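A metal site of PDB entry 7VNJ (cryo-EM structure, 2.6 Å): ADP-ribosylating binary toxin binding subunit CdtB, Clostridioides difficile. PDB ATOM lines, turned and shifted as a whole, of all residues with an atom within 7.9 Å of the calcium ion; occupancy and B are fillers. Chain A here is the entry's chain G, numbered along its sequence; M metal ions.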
ATOM      1  N   PHE A 418      18.341 -14.646   0.241  1.00  0.00           N
ATOM      2  CA  PHE A 418      18.436 -13.271   0.701  1.00  0.00           C
ATOM      3  C   PHE A 418      19.642 -13.127   1.622  1.00  0.00           C
ATOM      4  O   PHE A 418      19.897 -14.006   2.439  1.00  0.00           O
ATOM      5  CB  PHE A 418      17.151 -12.843   1.421  1.00  0.00           C
ATOM      6  CG  PHE A 418      17.254 -11.524   2.118  1.00  0.00           C
ATOM      7  CD1 PHE A 418      17.187 -10.338   1.394  1.00  0.00           C
ATOM      8  CD2 PHE A 418      17.407 -11.447   3.488  1.00  0.00           C
ATOM      9  CE1 PHE A 418      17.279  -9.125   2.029  1.00  0.00           C
ATOM     10  CE2 PHE A 418      17.498 -10.229   4.133  1.00  0.00           C
ATOM     11  CZ  PHE A 418      17.430  -9.072   3.399  1.00  0.00           C
ATOM     12  N   THR A 419      20.364 -12.025   1.473  1.00  0.00           N
ATOM     13  CA  THR A 419      21.463 -11.700   2.367  1.00  0.00           C
ATOM     14  C   THR A 419      21.411 -10.229   2.728  1.00  0.00           C
ATOM     15  O   THR A 419      21.079  -9.377   1.895  1.00  0.00           O
ATOM     16  CB  THR A 419      22.832 -12.040   1.735  1.00  0.00           C
ATOM     17  OG1 THR A 419      23.868 -11.681   2.653  1.00  0.00           O
ATOM     18  CG2 THR A 419      23.025 -11.287   0.435  1.00  0.00           C
ATOM     19  N   ASN A 420      21.714  -9.937   3.986  1.00  0.00           N
ATOM     20  CA  ASN A 420      21.843  -8.564   4.462  1.00  0.00           C
ATOM     21  C   ASN A 420      23.252  -8.278   4.966  1.00  0.00           C
ATOM     22  O   ASN A 420      23.505  -7.166   5.462  1.00  0.00           O
ATOM     23  CB  ASN A 420      20.830  -8.277   5.567  1.00  0.00           C
ATOM     24  CG  ASN A 420      21.038  -9.137   6.791  1.00  0.00           C
ATOM     25  OD1 ASN A 420      21.371 -10.315   6.681  1.00  0.00           O
ATOM     26  ND2 ASN A 420      20.840  -8.550   7.962  1.00  0.00           N
ATOM     27  N   PHE A 421      24.168  -9.238   4.865  1.00  0.00           N
ATOM     28  CA  PHE A 421      25.559  -9.135   5.299  1.00  0.00           C
ATOM     29  C   PHE A 421      25.704  -8.880   6.795  1.00  0.00           C
ATOM     30  O   PHE A 421      26.803  -8.570   7.255  1.00  0.00           O
ATOM     31  CB  PHE A 421      26.309  -8.055   4.510  1.00  0.00           C
ATOM     32  CG  PHE A 421      25.970  -8.014   3.049  1.00  0.00           C
ATOM     33  CD1 PHE A 421      26.276  -9.076   2.218  1.00  0.00           C
ATOM     34  CD2 PHE A 421      25.341  -6.907   2.506  1.00  0.00           C
ATOM     35  CE1 PHE A 421      25.958  -9.035   0.881  1.00  0.00           C
ATOM     36  CE2 PHE A 421      25.024  -6.871   1.160  1.00  0.00           C
ATOM     37  CZ  PHE A 421      25.332  -7.933   0.352  1.00  0.00           C
ATOM     38  N   ASP A 422      24.621  -8.999   7.565  1.00  0.00           N
ATOM     39  CA  ASP A 422      24.694  -8.857   9.008  1.00  0.00           C
ATOM     40  C   ASP A 422      24.318 -10.142   9.735  1.00  0.00           C
ATOM     41  O   ASP A 422      25.118 -10.636  10.546  1.00  0.00           O
ATOM     42  CB  ASP A 422      23.793  -7.699   9.472  1.00  0.00           C
ATOM     43  CG  ASP A 422      24.560  -6.406   9.624  1.00  0.00           C
ATOM     44  OD1 ASP A 422      25.743  -6.359   9.250  1.00  0.00           O
ATOM     45  OD2 ASP A 422      23.971  -5.432  10.142  1.00  0.00           O
ATOM     46  N   ASP A 423      23.140 -10.698   9.484  1.00  0.00           N
ATOM     47  CA  ASP A 423      22.661 -11.872  10.205  1.00  0.00           C
ATOM     48  C   ASP A 423      22.080 -12.957   9.328  1.00  0.00           C
ATOM     49  O   ASP A 423      22.015 -14.104   9.781  1.00  0.00           O
ATOM     50  CB  ASP A 423      21.599 -11.462  11.238  1.00  0.00           C
ATOM     51  CG  ASP A 423      21.940 -10.181  11.960  1.00  0.00           C
ATOM     52  OD1 ASP A 423      23.059 -10.089  12.512  1.00  0.00           O
ATOM     53  OD2 ASP A 423      21.087  -9.268  11.989  1.00  0.00           O
ATOM     54  N   THR A 436      32.303  -6.232   4.780  1.00  0.00           N
ATOM     55  CA  THR A 436      31.266  -5.743   5.668  1.00  0.00           C
ATOM     56  C   THR A 436      31.859  -5.125   6.929  1.00  0.00           C
ATOM     57  O   THR A 436      31.392  -5.342   8.045  1.00  0.00           O
ATOM     58  CB  THR A 436      30.294  -6.867   6.041  1.00  0.00           C
ATOM     59  OG1 THR A 436      30.903  -7.719   7.016  1.00  0.00           O
ATOM     60  CG2 THR A 436      29.928  -7.678   4.809  1.00  0.00           C
ATOM     61  N   ASN A 438      32.121  -1.844   7.575  1.00  0.00           N
ATOM     62  CA  ASN A 438      31.644  -0.496   7.805  1.00  0.00           C
ATOM     63  C   ASN A 438      30.135  -0.499   8.023  1.00  0.00           C
ATOM     64  O   ASN A 438      29.430  -1.438   7.655  1.00  0.00           O
ATOM     65  CB  ASN A 438      32.000   0.431   6.636  1.00  0.00           C
ATOM     66  CG  ASN A 438      31.648  -0.169   5.296  1.00  0.00           C
ATOM     67  OD1 ASN A 438      31.566  -1.384   5.149  1.00  0.00           O
ATOM     68  ND2 ASN A 438      31.440   0.684   4.296  1.00  0.00           N
ATOM     69  N   ASP A 440      27.046   0.690   6.823  1.00  0.00           N
ATOM     70  CA  ASP A 440      26.349   1.233   5.676  1.00  0.00           C
ATOM     71  C   ASP A 440      25.181   0.295   5.361  1.00  0.00           C
ATOM     72  O   ASP A 440      24.825  -0.570   6.157  1.00  0.00           O
ATOM     73  CB  ASP A 440      27.301   1.410   4.482  1.00  0.00           C
ATOM     74  CG  ASP A 440      28.324   2.504   4.724  1.00  0.00           C
ATOM     75  OD1 ASP A 440      27.918   3.677   4.832  1.00  0.00           O
ATOM     76  OD2 ASP A 440      29.524   2.179   4.802  1.00  0.00           O
ATOM     77  N   GLY A 441      24.581   0.484   4.187  1.00  0.00           N
ATOM     78  CA  GLY A 441      23.422  -0.299   3.844  1.00  0.00           C
ATOM     79  C   GLY A 441      22.201   0.173   4.626  1.00  0.00           C
ATOM     80  O   GLY A 441      22.245   1.149   5.368  1.00  0.00           O
ATOM     81  N   LEU A 442      21.107  -0.550   4.426  1.00  0.00           N
ATOM     82  CA  LEU A 442      19.903  -0.257   5.193  1.00  0.00           C
ATOM     83  C   LEU A 442      20.126  -0.509   6.677  1.00  0.00           C
ATOM     84  O   LEU A 442      19.666   0.263   7.520  1.00  0.00           O
ATOM     85  CB  LEU A 442      18.720  -1.076   4.677  1.00  0.00           C
ATOM     86  CG  LEU A 442      17.920  -0.487   3.512  1.00  0.00           C
ATOM     87  CD1 LEU A 442      17.320   0.861   3.910  1.00  0.00           C
ATOM     88  CD2 LEU A 442      18.745  -0.356   2.252  1.00  0.00           C
ATOM     89  N   GLN A 443      20.832  -1.583   7.011  1.00  0.00           N
ATOM     90  CA  GLN A 443      21.148  -1.914   8.406  1.00  0.00           C
ATOM     91  C   GLN A 443      22.587  -2.408   8.481  1.00  0.00           C
ATOM     92  O   GLN A 443      22.845  -3.612   8.377  1.00  0.00           O
ATOM     93  CB  GLN A 443      20.168  -2.937   8.964  1.00  0.00           C
ATOM     94  CG  GLN A 443      18.734  -2.443   9.077  1.00  0.00           C
ATOM     95  CD  GLN A 443      17.846  -2.968   7.972  1.00  0.00           C
ATOM     96  OE1 GLN A 443      17.997  -4.104   7.518  1.00  0.00           O
ATOM     97  NE2 GLN A 443      16.910  -2.149   7.518  1.00  0.00           N
ATOM     98  N   GLY A 444      23.523  -1.478   8.650  1.00  0.00           N
ATOM     99  CA  GLY A 444      24.883  -1.782   9.073  1.00  0.00           C
ATOM    100  C   GLY A 444      25.694  -2.766   8.244  1.00  0.00           C
ATOM    101  O   GLY A 444      26.344  -3.653   8.808  1.00  0.00           O
ATOM    102  N   SER A 445      25.701  -2.620   6.915  1.00  0.00           N
ATOM    103  CA  SER A 445      26.486  -3.507   6.062  1.00  0.00           C
ATOM    104  C   SER A 445      26.583  -2.898   4.668  1.00  0.00           C
ATOM    105  O   SER A 445      25.575  -2.446   4.126  1.00  0.00           O
ATOM    106  CB  SER A 445      25.843  -4.893   5.985  1.00  0.00           C
ATOM    107  OG  SER A 445      24.810  -4.933   5.018  1.00  0.00           O
ATOM    108  N   ALA A 446      27.787  -2.932   4.090  1.00  0.00           N
ATOM    109  CA  ALA A 446      28.032  -2.294   2.804  1.00  0.00           C
ATOM    110  C   ALA A 446      28.264  -3.302   1.688  1.00  0.00           C
ATOM    111  O   ALA A 446      27.547  -3.285   0.685  1.00  0.00           O
ATOM    112  CB  ALA A 446      29.230  -1.340   2.915  1.00  0.00           C
ATOM    113  N   ASN A 447      29.251  -4.189   1.846  1.00  0.00           N
ATOM    114  CA  ASN A 447      29.556  -5.227   0.849  1.00  0.00           C
ATOM    115  C   ASN A 447      29.814  -4.620  -0.532  1.00  0.00           C
ATOM    116  O   ASN A 447      29.053  -4.828  -1.477  1.00  0.00           O
ATOM    117  CB  ASN A 447      28.448  -6.271   0.799  1.00  0.00           C
ATOM    118  CG  ASN A 447      28.758  -7.408  -0.163  1.00  0.00           C
ATOM    119  OD1 ASN A 447      29.594  -8.256   0.120  1.00  0.00           O
ATOM    120  ND2 ASN A 447      28.088  -7.408  -1.309  1.00  0.00           N
ATOM    121  N   LEU A 532      25.710  -1.150  -1.557  1.00  0.00           N
ATOM    122  CA  LEU A 532      24.748  -2.225  -1.760  1.00  0.00           C
ATOM    123  C   LEU A 532      24.254  -2.742  -0.417  1.00  0.00           C
ATOM    124  O   LEU A 532      24.911  -2.581   0.609  1.00  0.00           O
ATOM    125  CB  LEU A 532      25.366  -3.384  -2.554  1.00  0.00           C
ATOM    126  CG  LEU A 532      25.760  -3.126  -4.005  1.00  0.00           C
ATOM    127  CD1 LEU A 532      26.471  -4.337  -4.547  1.00  0.00           C
ATOM    128  CD2 LEU A 532      24.547  -2.801  -4.858  1.00  0.00           C
ATOM    129  N   ASP A 533      23.083  -3.387  -0.449  1.00  0.00           N
ATOM    130  CA  ASP A 533      22.537  -4.109   0.688  1.00  0.00           C
ATOM    131  C   ASP A 533      21.263  -4.829   0.252  1.00  0.00           C
ATOM    132  O   ASP A 533      20.621  -4.438  -0.721  1.00  0.00           O
ATOM    133  CB  ASP A 533      22.226  -3.192   1.873  1.00  0.00           C
ATOM    134  CG  ASP A 533      22.414  -3.873   3.212  1.00  0.00           C
ATOM    135  OD1 ASP A 533      22.763  -5.068   3.221  1.00  0.00           O
ATOM    136  OD2 ASP A 533      22.217  -3.229   4.257  1.00  0.00           O
ATOM    137  N   ASN A 534      20.927  -5.893   0.988  1.00  0.00           N
ATOM    138  CA  ASN A 534      19.655  -6.608   0.848  1.00  0.00           C
ATOM    139  C   ASN A 534      19.447  -7.123  -0.576  1.00  0.00           C
ATOM    140  O   ASN A 534      18.498  -6.755  -1.262  1.00  0.00           O
ATOM    141  CB  ASN A 534      18.493  -5.713   1.293  1.00  0.00           C
ATOM    142  CG  ASN A 534      18.486  -5.449   2.784  1.00  0.00           C
ATOM    143  OD1 ASN A 534      18.959  -6.261   3.565  1.00  0.00           O
ATOM    144  ND2 ASN A 534      17.945  -4.307   3.173  1.00  0.00           N
HETATM  145 CA    CA M   1      22.716  -4.762   6.183  1.00  0.00          CA
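The backbone NH (N) of Leu 442 sits close to the side-chain carboxylate (OD2) of Asp 533. The backbone NH (N) of Asp 423 sits at hydrogen-bond distance from the side-chain amide oxygen (OD1) of Asn 420, 3.3 Å away.
Of the 19 residues printed, 4 come within 4 Å of the calcium ion.
The calcium ion is bound by the side-chain hydroxyl (OG) of Ser 445 (2.4 Å), the backbone carbonyl oxygen (O) of Gln 443 (2.5 Å), the side-chain carboxylate (OD2) of Asp 533 (2.5 Å) and the backbone carbonyl oxygen (O) of Asn 420 (2.6 Å). Slightly farther from the calcium ion lies the side-chain carboxylate (OD1) of Asp 533 (3.0 Å).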
